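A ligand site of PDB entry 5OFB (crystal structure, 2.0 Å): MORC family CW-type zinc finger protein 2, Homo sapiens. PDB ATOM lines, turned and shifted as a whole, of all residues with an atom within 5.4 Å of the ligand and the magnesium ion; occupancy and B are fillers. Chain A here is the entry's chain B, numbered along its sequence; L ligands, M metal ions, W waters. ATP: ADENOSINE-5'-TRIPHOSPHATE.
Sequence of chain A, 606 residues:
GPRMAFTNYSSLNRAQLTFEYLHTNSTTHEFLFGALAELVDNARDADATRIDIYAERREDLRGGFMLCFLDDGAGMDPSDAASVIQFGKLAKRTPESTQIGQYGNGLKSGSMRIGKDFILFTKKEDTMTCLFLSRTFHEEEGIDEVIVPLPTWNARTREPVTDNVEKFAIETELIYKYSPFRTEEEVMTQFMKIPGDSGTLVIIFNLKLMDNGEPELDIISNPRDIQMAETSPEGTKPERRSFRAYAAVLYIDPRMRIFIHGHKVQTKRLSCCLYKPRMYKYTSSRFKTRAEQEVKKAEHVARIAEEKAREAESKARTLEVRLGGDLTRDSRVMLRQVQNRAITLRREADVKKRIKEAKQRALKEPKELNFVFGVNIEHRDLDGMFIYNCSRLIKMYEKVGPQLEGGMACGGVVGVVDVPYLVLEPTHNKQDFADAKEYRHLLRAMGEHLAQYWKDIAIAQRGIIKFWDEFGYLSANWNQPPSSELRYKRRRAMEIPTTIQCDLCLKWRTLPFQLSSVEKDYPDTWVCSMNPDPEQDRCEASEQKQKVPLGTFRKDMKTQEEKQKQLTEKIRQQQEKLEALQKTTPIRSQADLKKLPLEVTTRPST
The backbone NH of Tyr 103 lies within hydrogen-bond range of an oxygen (O3G) of the ligand (3.0 Å). N1 of the ligand sits at hydrogen-bond distance from OG1 of Thr 200. The backbone NH (N) of Asn 105 lies within hydrogen-bond range of an oxygen (O2G) of the ligand (2.8 Å). The backbone NH (N) of Gly 104 sits at hydrogen-bond distance from an oxygen (O3B) of the ligand (3.0 Å). O1A of the ligand is in salt-bridge range of NZ of Lys 108 (2.7 Å). The backbone NH (N) of Leu 107 sits at hydrogen-bond distance from an oxygen (O1A) of the ligand (3.2 Å). The side-chain carboxylate (OD2) of Asp 71 is in hydrogen-bond range of a nitrogen (N6) of the ligand (2.8 Å). The backbone NH (N) of Gly 106 lies within hydrogen-bond range of an oxygen (O2G) of the ligand (2.9 Å). N of Gln 102 is in hydrogen-bond range of O3G of the ligand (2.8 Å). NZ of Lys 430 is in salt-bridge range of O3G of the ligand (2.6 Å). NZ of Lys 89 is in salt-bridge range of O1B of the ligand (3.1 Å).
The side-chain amino group (NZ) of Lys 108 is in hydrogen-bond range of the backbone carbonyl oxygen (O) of Val 84, at 2.8 Å. The backbone carbonyl oxygen (O) of Gly 104 lies within hydrogen-bond range of the side-chain amino group (NZ) of Lys 108. The backbone NH (N) of Ile 100 sits at hydrogen-bond distance from the side-chain carboxylate (OD1) of Asp 45 (2.8 Å). The backbone NH (N) of Asp 71 is in hydrogen-bond range of the backbone carbonyl oxygen (O) of Thr 200 (2.9 Å). The backbone NH (N) of Gly 101 is in hydrogen-bond range of the side-chain carboxylate (OD2) of Asp 45 (2.8 Å). The side-chain amino group (NZ) of Lys 430 is in hydrogen-bond range of the backbone carbonyl oxygen (O) of Ile 100 (3.1 Å).
The side-chain carboxylate (OE2) of Glu 38 lies close to an oxygen (O1G) of the ligand (3.5 Å). SD of Met 76 lies close to N3 of the ligand (3.6 Å). Ala 43 touches the ligand (N to N6, 3.96 Å). Ala 46 touches the ligand (CB to N1, 3.4 Å). Val 84 touches the ligand. Ile 100 touches the ligand (O to O3G, 3.9 Å). Gly 101 touches the ligand (CA to O3G, 3.3 Å). Hydrophobic or aromatic side chains within 4 Å of the ligand: Ala 46, Met 76, Val 84, Tyr 103 and Leu 107. The nearest printed residue that does not touch the ligand is Gly 75 (4.1 Å).
Within 4 Å of the magnesium ion: Asn 42. The nearest printed residue that does not touch the magnesium ion is Glu 38 (4.1 Å).
O1G of the ligand binds the magnesium ion (1.9 Å). An oxygen (O2B) of the ligand binds the magnesium ion (2.0 Å). The magnesium ion is bound by the side-chain amide oxygen (OD1) of Asn 42 (2.1 Å). Water W1 is bound to the magnesium ion, 2.1 Å away. O2A of the ligand is bound to the magnesium ion, 2.2 Å away. Water W10 is bound to the magnesium ion, 2.2 Å away.
Water W1 lies within hydrogen-bond range of OD2 of Asp 45 (3.2 Å) and N of Gly 101 (3.4 Å). Water W8 bridges an oxygen (O2') of the ligand and the side-chain amino group of Lys 89. Water W5 lies within hydrogen-bond range of the side-chain carboxylate (OD1) of Asp 71 (2.7 Å), the side-chain hydroxyl (OG1) of Thr 200 (2.7 Å), a nitrogen (N1) of the ligand (2.8 Å) and the backbone NH (N) of Gly 75 (2.9 Å). Water W7 lies within hydrogen-bond range of an oxygen (O2G) of the ligand (2.9 Å), the side-chain carboxylate (OE1) of Glu 38 (3.2 Å) and the backbone NH (N) of Gly 106 (3.5 Å). Water W9 bridges O of Leu 39 (2.8 Å) and N6 of the ligand (3.1 Å). Water W4 lies within hydrogen-bond range of OE2 of Glu 38 (2.5 Å), OD2 of Asp 41 (2.7 Å) and NZ of Lys 430 (2.8 Å).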
ATOM      1  N   GLU A  38      12.752  -5.150  17.129  1.00  0.00           N
ATOM      2  CA  GLU A  38      12.638  -6.600  17.163  1.00  0.00           C
ATOM      3  C   GLU A  38      14.020  -7.278  17.076  1.00  0.00           C
ATOM      4  O   GLU A  38      14.317  -8.234  17.790  1.00  0.00           O
ATOM      5  CB  GLU A  38      11.758  -7.125  16.019  1.00  0.00           C
ATOM      6  CG  GLU A  38      10.255  -6.802  16.161  1.00  0.00           C
ATOM      7  CD  GLU A  38       9.580  -7.648  17.263  1.00  0.00           C
ATOM      8  OE1 GLU A  38       8.315  -7.670  17.269  1.00  0.00           O
ATOM      9  OE2 GLU A  38      10.276  -8.340  18.136  1.00  0.00           O
ATOM     10  N   LEU A  39      14.896  -6.744  16.212  1.00  0.00           N
ATOM     11  CA  LEU A  39      16.205  -7.365  16.045  1.00  0.00           C
ATOM     12  C   LEU A  39      17.143  -7.086  17.230  1.00  0.00           C
ATOM     13  O   LEU A  39      17.955  -7.910  17.614  1.00  0.00           O
ATOM     14  CB  LEU A  39      16.830  -6.877  14.718  1.00  0.00           C
ATOM     15  CG  LEU A  39      16.150  -7.525  13.493  1.00  0.00           C
ATOM     16  CD1 LEU A  39      14.916  -6.775  13.033  1.00  0.00           C
ATOM     17  CD2 LEU A  39      17.136  -7.575  12.346  1.00  0.00           C
ATOM     18  N   ASP A  41      15.974  -6.732  20.303  1.00  0.00           N
ATOM     19  CA  ASP A  41      15.428  -7.666  21.309  1.00  0.00           C
ATOM     20  C   ASP A  41      16.019  -9.072  21.157  1.00  0.00           C
ATOM     21  O   ASP A  41      16.303  -9.728  22.145  1.00  0.00           O
ATOM     22  CB  ASP A  41      13.929  -7.869  21.160  1.00  0.00           C
ATOM     23  CG  ASP A  41      13.077  -6.594  21.457  1.00  0.00           C
ATOM     24  OD1 ASP A  41      13.505  -5.602  22.036  1.00  0.00           O
ATOM     25  OD2 ASP A  41      11.883  -6.575  21.146  1.00  0.00           O
ATOM     26  N   ASN A  42      16.106  -9.561  19.942  1.00  0.00           N
ATOM     27  CA  ASN A  42      16.708 -10.884  19.730  1.00  0.00           C
ATOM     28  C   ASN A  42      18.152 -10.995  20.202  1.00  0.00           C
ATOM     29  O   ASN A  42      18.517 -12.059  20.702  1.00  0.00           O
ATOM     30  CB  ASN A  42      16.627 -11.307  18.280  1.00  0.00           C
ATOM     31  CG  ASN A  42      15.198 -11.600  17.815  1.00  0.00           C
ATOM     32  OD1 ASN A  42      14.283 -11.882  18.613  1.00  0.00           O
ATOM     33  ND2 ASN A  42      15.019 -11.569  16.532  1.00  0.00           N
ATOM     34  N   ALA A  43      18.988  -9.949  19.953  1.00  0.00           N
ATOM     35  CA  ALA A  43      20.345  -9.907  20.491  1.00  0.00           C
ATOM     36  C   ALA A  43      20.340  -9.893  22.033  1.00  0.00           C
ATOM     37  O   ALA A  43      21.078 -10.634  22.675  1.00  0.00           O
ATOM     38  CB  ALA A  43      21.111  -8.680  19.959  1.00  0.00           C
ATOM     39  N   ASP A  45      18.014 -11.068  24.038  1.00  0.00           N
ATOM     40  CA  ASP A  45      17.566 -12.420  24.460  1.00  0.00           C
ATOM     41  C   ASP A  45      18.677 -13.462  24.284  1.00  0.00           C
ATOM     42  O   ASP A  45      18.690 -14.445  25.017  1.00  0.00           O
ATOM     43  CB  ASP A  45      16.368 -12.890  23.650  1.00  0.00           C
ATOM     44  CG  ASP A  45      15.044 -12.182  24.021  1.00  0.00           C
ATOM     45  OD1 ASP A  45      14.926 -11.654  25.155  1.00  0.00           O
ATOM     46  OD2 ASP A  45      14.108 -12.274  23.165  1.00  0.00           O
ATOM     47  N   ALA A  46      19.591 -13.261  23.329  1.00  0.00           N
ATOM     48  CA  ALA A  46      20.706 -14.184  23.158  1.00  0.00           C
ATOM     49  C   ALA A  46      21.910 -13.907  24.077  1.00  0.00           C
ATOM     50  O   ALA A  46      22.995 -14.426  23.829  1.00  0.00           O
ATOM     51  CB  ALA A  46      21.130 -14.182  21.723  1.00  0.00           C
ATOM     52  N   ASP A  71      25.743  -8.942  16.680  1.00  0.00           N
ATOM     53  CA  ASP A  71      25.810  -9.167  18.124  1.00  0.00           C
ATOM     54  C   ASP A  71      26.828 -10.261  18.484  1.00  0.00           C
ATOM     55  O   ASP A  71      27.147 -11.111  17.646  1.00  0.00           O
ATOM     56  CB  ASP A  71      24.451  -9.454  18.697  1.00  0.00           C
ATOM     57  CG  ASP A  71      23.882 -10.831  18.357  1.00  0.00           C
ATOM     58  OD1 ASP A  71      24.447 -11.915  18.697  1.00  0.00           O
ATOM     59  OD2 ASP A  71      22.776 -10.898  17.793  1.00  0.00           O
ATOM     60  N   GLY A  75      24.550 -17.020  19.563  1.00  0.00           N
ATOM     61  CA  GLY A  75      24.545 -17.622  18.251  1.00  0.00           C
ATOM     62  C   GLY A  75      23.543 -18.785  18.202  1.00  0.00           C
ATOM     63  O   GLY A  75      22.756 -18.997  19.140  1.00  0.00           O
ATOM     64  N   MET A  76      23.520 -19.484  17.089  1.00  0.00           N
ATOM     65  CA  MET A  76      22.573 -20.572  16.834  1.00  0.00           C
ATOM     66  C   MET A  76      23.298 -21.744  16.193  1.00  0.00           C
ATOM     67  O   MET A  76      24.035 -21.545  15.236  1.00  0.00           O
ATOM     68  CB  MET A  76      21.495 -20.078  15.885  1.00  0.00           C
ATOM     69  CG  MET A  76      20.458 -19.148  16.609  1.00  0.00           C
ATOM     70  SD  MET A  76      19.244 -18.523  15.440  1.00  0.00           S
ATOM     71  CE  MET A  76      20.157 -17.169  14.677  1.00  0.00           C
ATOM     72  N   ASP A  80      18.656 -24.677  15.714  1.00  0.00           N
ATOM     73  CA  ASP A  80      18.175 -23.371  16.177  1.00  0.00           C
ATOM     74  C   ASP A  80      17.917 -22.486  14.930  1.00  0.00           C
ATOM     75  O   ASP A  80      16.901 -21.844  14.817  1.00  0.00           O
ATOM     76  CB  ASP A  80      19.208 -22.620  17.073  1.00  0.00           C
ATOM     77  CG  ASP A  80      19.608 -23.383  18.371  1.00  0.00           C
ATOM     78  OD1 ASP A  80      18.705 -24.064  18.939  1.00  0.00           O
ATOM     79  OD2 ASP A  80      20.824 -23.237  18.835  1.00  0.00           O
ATOM     80  N   SER A  83      14.753 -23.202  13.089  1.00  0.00           N
ATOM     81  CA  SER A  83      13.521 -22.775  13.761  1.00  0.00           C
ATOM     82  C   SER A  83      13.276 -21.253  13.637  1.00  0.00           C
ATOM     83  O   SER A  83      12.207 -20.733  13.968  1.00  0.00           O
ATOM     84  CB  SER A  83      13.519 -23.263  15.199  1.00  0.00           C
ATOM     85  OG  SER A  83      14.209 -22.350  16.002  1.00  0.00           O
ATOM     86  N   VAL A  84      14.247 -20.510  13.113  1.00  0.00           N
ATOM     87  CA  VAL A  84      14.009 -19.094  12.858  1.00  0.00           C
ATOM     88  C   VAL A  84      12.819 -18.837  11.933  1.00  0.00           C
ATOM     89  O   VAL A  84      12.036 -17.901  12.176  1.00  0.00           O
ATOM     90  CB  VAL A  84      15.232 -18.425  12.293  1.00  0.00           C
ATOM     91  CG1 VAL A  84      14.947 -16.991  11.926  1.00  0.00           C
ATOM     92  CG2 VAL A  84      16.371 -18.461  13.292  1.00  0.00           C
ATOM     93  N   LYS A  89       6.215 -20.085  18.182  1.00  0.00           N
ATOM     94  CA  LYS A  89       7.127 -21.001  18.864  1.00  0.00           C
ATOM     95  C   LYS A  89       6.347 -22.309  19.169  1.00  0.00           C
ATOM     96  O   LYS A  89       5.157 -22.478  18.830  1.00  0.00           O
ATOM     97  CB  LYS A  89       7.566 -20.365  20.149  1.00  0.00           C
ATOM     98  CG  LYS A  89       8.306 -19.060  19.909  1.00  0.00           C
ATOM     99  CD  LYS A  89       8.685 -18.482  21.257  1.00  0.00           C
ATOM    100  CE  LYS A  89      10.166 -18.249  21.540  1.00  0.00           C
ATOM    101  NZ  LYS A  89      11.071 -18.991  20.666  1.00  0.00           N
ATOM    102  N   ILE A 100      12.292 -11.679  26.137  1.00  0.00           N
ATOM    103  CA  ILE A 100      11.356 -10.802  25.409  1.00  0.00           C
ATOM    104  C   ILE A 100      10.626 -11.606  24.347  1.00  0.00           C
ATOM    105  O   ILE A 100       9.434 -11.448  24.164  1.00  0.00           O
ATOM    106  CB  ILE A 100      12.096  -9.564  24.832  1.00  0.00           C
ATOM    107  CG1 ILE A 100      12.652  -8.726  26.014  1.00  0.00           C
ATOM    108  CG2 ILE A 100      11.153  -8.687  23.976  1.00  0.00           C
ATOM    109  CD1 ILE A 100      13.708  -7.695  25.680  1.00  0.00           C
ATOM    110  N   GLY A 101      11.358 -12.456  23.601  1.00  0.00           N
ATOM    111  CA  GLY A 101      10.786 -13.256  22.508  1.00  0.00           C
ATOM    112  C   GLY A 101       9.827 -14.333  22.990  1.00  0.00           C
ATOM    113  O   GLY A 101      10.207 -15.198  23.810  1.00  0.00           O
ATOM    114  N   GLN A 102       8.558 -14.234  22.599  1.00  0.00           N
ATOM    115  CA  GLN A 102       7.554 -15.224  22.945  1.00  0.00           C
ATOM    116  C   GLN A 102       6.683 -15.604  21.762  1.00  0.00           C
ATOM    117  O   GLN A 102       6.140 -16.683  21.739  1.00  0.00           O
ATOM    118  CB  GLN A 102       6.659 -14.737  24.106  1.00  0.00           C
ATOM    119  CG  GLN A 102       7.364 -14.330  25.422  1.00  0.00           C
ATOM    120  CD  GLN A 102       7.957 -15.538  26.219  1.00  0.00           C
ATOM    121  OE1 GLN A 102       7.400 -16.626  26.184  1.00  0.00           O
ATOM    122  NE2 GLN A 102       9.102 -15.338  26.890  1.00  0.00           N
ATOM    123  N   TYR A 103       6.560 -14.723  20.755  1.00  0.00           N
ATOM    124  CA  TYR A 103       5.621 -14.876  19.677  1.00  0.00           C
ATOM    125  C   TYR A 103       6.120 -15.569  18.428  1.00  0.00           C
ATOM    126  O   TYR A 103       5.318 -16.003  17.549  1.00  0.00           O
ATOM    127  CB  TYR A 103       5.011 -13.512  19.308  1.00  0.00           C
ATOM    128  CG  TYR A 103       4.121 -12.897  20.330  1.00  0.00           C
ATOM    129  CD1 TYR A 103       3.530 -13.642  21.394  1.00  0.00           C
ATOM    130  CD2 TYR A 103       3.778 -11.523  20.226  1.00  0.00           C
ATOM    131  CE1 TYR A 103       2.759 -12.997  22.343  1.00  0.00           C
ATOM    132  CE2 TYR A 103       2.914 -10.921  21.129  1.00  0.00           C
ATOM    133  CZ  TYR A 103       2.438 -11.661  22.177  1.00  0.00           C
ATOM    134  OH  TYR A 103       1.632 -11.055  23.112  1.00  0.00           O
ATOM    135  N   GLY A 104       7.404 -15.796  18.356  1.00  0.00           N
ATOM    136  CA  GLY A 104       7.989 -16.479  17.255  1.00  0.00           C
ATOM    137  C   GLY A 104       7.843 -15.774  15.902  1.00  0.00           C
ATOM    138  O   GLY A 104       7.676 -16.419  14.860  1.00  0.00           O
ATOM    139  N   ASN A 105       7.937 -14.460  15.894  1.00  0.00           N
ATOM    140  CA  ASN A 105       7.549 -13.680  14.724  1.00  0.00           C
ATOM    141  C   ASN A 105       8.407 -12.419  14.469  1.00  0.00           C
ATOM    142  O   ASN A 105       8.500 -11.986  13.295  1.00  0.00           O
ATOM    143  CB  ASN A 105       6.072 -13.191  14.946  1.00  0.00           C
ATOM    144  CG  ASN A 105       5.441 -12.647  13.673  1.00  0.00           C
ATOM    145  OD1 ASN A 105       5.647 -13.205  12.616  1.00  0.00           O
ATOM    146  ND2 ASN A 105       4.727 -11.569  13.779  1.00  0.00           N
ATOM    147  N   GLY A 106       8.992 -11.835  15.511  1.00  0.00           N
ATOM    148  CA  GLY A 106       9.575 -10.474  15.423  1.00  0.00           C
ATOM    149  C   GLY A 106      10.583 -10.257  14.349  1.00  0.00           C
ATOM    150  O   GLY A 106      10.583  -9.262  13.693  1.00  0.00           O
ATOM    151  N   LEU A 107      11.506 -11.191  14.165  1.00  0.00           N
ATOM    152  CA  LEU A 107      12.485 -11.021  13.162  1.00  0.00           C
ATOM    153  C   LEU A 107      11.844 -10.984  11.751  1.00  0.00           C
ATOM    154  O   LEU A 107      12.282 -10.223  10.883  1.00  0.00           O
ATOM    155  CB  LEU A 107      13.488 -12.171  13.209  1.00  0.00           C
ATOM    156  CG  LEU A 107      14.480 -12.282  12.069  1.00  0.00           C
ATOM    157  CD1 LEU A 107      15.353 -11.041  11.847  1.00  0.00           C
ATOM    158  CD2 LEU A 107      15.383 -13.503  12.302  1.00  0.00           C
ATOM    159  N   LYS A 108      10.807 -11.761  11.525  1.00  0.00           N
ATOM    160  CA  LYS A 108      10.167 -11.778  10.222  1.00  0.00           C
ATOM    161  C   LYS A 108       9.290 -10.531  10.042  1.00  0.00           C
ATOM    162  O   LYS A 108       9.364  -9.912   9.000  1.00  0.00           O
ATOM    163  CB  LYS A 108       9.366 -13.068  10.027  1.00  0.00           C
ATOM    164  CG  LYS A 108      10.275 -14.286   9.928  1.00  0.00           C
ATOM    165  CD  LYS A 108      10.756 -14.863  11.295  1.00  0.00           C
ATOM    166  CE  LYS A 108       9.657 -15.601  12.045  1.00  0.00           C
ATOM    167  NZ  LYS A 108      10.170 -16.204  13.327  1.00  0.00           N
ATOM    168  N   LEU A 120      21.062 -13.776   7.079  1.00  0.00           N
ATOM    169  CA  LEU A 120      21.528 -13.859   8.452  1.00  0.00           C
ATOM    170  C   LEU A 120      22.711 -14.851   8.514  1.00  0.00           C
ATOM    171  O   LEU A 120      22.718 -15.874   7.823  1.00  0.00           O
ATOM    172  CB  LEU A 120      20.385 -14.315   9.338  1.00  0.00           C
ATOM    173  CG  LEU A 120      20.600 -14.721  10.805  1.00  0.00           C
ATOM    174  CD1 LEU A 120      19.251 -14.586  11.481  1.00  0.00           C
ATOM    175  CD2 LEU A 120      21.124 -16.139  10.976  1.00  0.00           C
ATOM    176  N   THR A 200      25.740 -13.450  15.927  1.00  0.00           N
ATOM    177  CA  THR A 200      24.853 -13.414  14.830  1.00  0.00           C
ATOM    178  C   THR A 200      24.959 -12.054  14.142  1.00  0.00           C
ATOM    179  O   THR A 200      25.028 -11.005  14.811  1.00  0.00           O
ATOM    180  CB  THR A 200      23.392 -13.663  15.286  1.00  0.00           C
ATOM    181  OG1 THR A 200      23.287 -14.941  15.957  1.00  0.00           O
ATOM    182  CG2 THR A 200      22.448 -13.591  14.156  1.00  0.00           C
ATOM    183  N   VAL A 202      22.759 -10.045  11.178  1.00  0.00           N
ATOM    184  CA  VAL A 202      21.579  -9.977  10.353  1.00  0.00           C
ATOM    185  C   VAL A 202      21.735  -8.775   9.427  1.00  0.00           C
ATOM    186  O   VAL A 202      21.963  -7.654   9.878  1.00  0.00           O
ATOM    187  CB  VAL A 202      20.282  -9.798  11.192  1.00  0.00           C
ATOM    188  CG1 VAL A 202      19.033  -9.923  10.324  1.00  0.00           C
ATOM    189  CG2 VAL A 202      20.238 -10.763  12.368  1.00  0.00           C
ATOM    190  N   LYS A 430       4.367  -5.266  19.260  1.00  0.00           N
ATOM    191  CA  LYS A 430       5.066  -4.863  20.484  1.00  0.00           C
ATOM    192  C   LYS A 430       5.130  -3.352  20.646  1.00  0.00           C
ATOM    193  O   LYS A 430       6.087  -2.830  21.177  1.00  0.00           O
ATOM    194  CB  LYS A 430       6.450  -5.533  20.626  1.00  0.00           C
ATOM    195  CG  LYS A 430       6.319  -7.066  20.506  1.00  0.00           C
ATOM    196  CD  LYS A 430       7.347  -7.813  21.302  1.00  0.00           C
ATOM    197  CE  LYS A 430       7.171  -9.341  21.075  1.00  0.00           C
ATOM    198  NZ  LYS A 430       8.350 -10.022  21.646  1.00  0.00           N
HETATM  199  PG  ATP L   1       9.123 -12.574  19.186  1.00  0.00           P
HETATM  200  O1G ATP L   1      10.325 -11.716  18.890  1.00  0.00           O
HETATM  201  O2G ATP L   1       8.183 -12.776  18.079  1.00  0.00           O
HETATM  202  O3G ATP L   1       8.367 -12.335  20.503  1.00  0.00           O
HETATM  203  PB  ATP L   1      11.113 -14.697  18.958  1.00  0.00           P
HETATM  204  O1B ATP L   1      11.092 -16.103  19.464  1.00  0.00           O
HETATM  205  O2B ATP L   1      12.263 -13.823  19.320  1.00  0.00           O
HETATM  206  O3B ATP L   1       9.699 -14.086  19.405  1.00  0.00           O
HETATM  207  PA  ATP L   1      11.891 -14.102  16.269  1.00  0.00           P
HETATM  208  O1A ATP L   1      11.213 -14.311  14.990  1.00  0.00           O
HETATM  209  O2A ATP L   1      12.231 -12.727  16.768  1.00  0.00           O
HETATM  210  O3A ATP L   1      10.887 -14.770  17.332  1.00  0.00           O
HETATM  211  O5' ATP L   1      13.225 -15.034  16.316  1.00  0.00           O
HETATM  212  C5' ATP L   1      13.059 -16.409  16.078  1.00  0.00           C
HETATM  213  C4' ATP L   1      14.142 -17.201  16.777  1.00  0.00           C
HETATM  214  O4' ATP L   1      15.393 -16.967  16.146  1.00  0.00           O
HETATM  215  C3' ATP L   1      14.371 -16.758  18.213  1.00  0.00           C
HETATM  216  O3' ATP L   1      13.431 -17.476  19.004  1.00  0.00           O
HETATM  217  C2' ATP L   1      15.791 -17.152  18.440  1.00  0.00           C
HETATM  218  O2' ATP L   1      15.695 -18.550  18.737  1.00  0.00           O
HETATM  219  C1' ATP L   1      16.445 -16.960  17.074  1.00  0.00           C
HETATM  220  N9  ATP L   1      17.175 -15.690  16.923  1.00  0.00           N
HETATM  221  C8  ATP L   1      16.800 -14.613  16.187  1.00  0.00           C
HETATM  222  N7  ATP L   1      17.742 -13.655  16.242  1.00  0.00           N
HETATM  223  C5  ATP L   1      18.735 -14.143  17.027  1.00  0.00           C
HETATM  224  C6  ATP L   1      20.038 -13.630  17.514  1.00  0.00           C
HETATM  225  N6  ATP L   1      20.442 -12.380  17.188  1.00  0.00           N
HETATM  226  N1  ATP L   1      20.777 -14.445  18.315  1.00  0.00           N
HETATM  227  C2  ATP L   1      20.384 -15.699  18.632  1.00  0.00           C
HETATM  228  N3  ATP L   1      19.216 -16.230  18.227  1.00  0.00           N
HETATM  229  C4  ATP L   1      18.364 -15.485  17.456  1.00  0.00           C
HETATM  230 MG    MG M   1      12.219 -11.902  18.758  1.00  0.00          MG
HETATM  231  O   HOH W   1      12.504 -11.094  20.662  1.00  0.00           O
HETATM  232  O   HOH W   2      17.235 -11.179  14.821  1.00  0.00           O
HETATM  233  O   HOH W   3      17.160 -14.285  20.421  1.00  0.00           O
HETATM  234  O   HOH W   4      10.653  -8.917  20.589  1.00  0.00           O
HETATM  235  O   HOH W   5      23.572 -14.424  18.598  1.00  0.00           O
HETATM  236  O   HOH W   6      14.375 -14.103  21.192  1.00  0.00           O
HETATM  237  O   HOH W   7       6.630 -10.360  17.601  1.00  0.00           O
HETATM  238  O   HOH W   8      14.510 -18.786  21.148  1.00  0.00           O
HETATM  239  O   HOH W   9      19.371  -9.708  15.982  1.00  0.00           O
HETATM  240  O   HOH W  10      12.255 -10.013  17.705  1.00  0.00           O
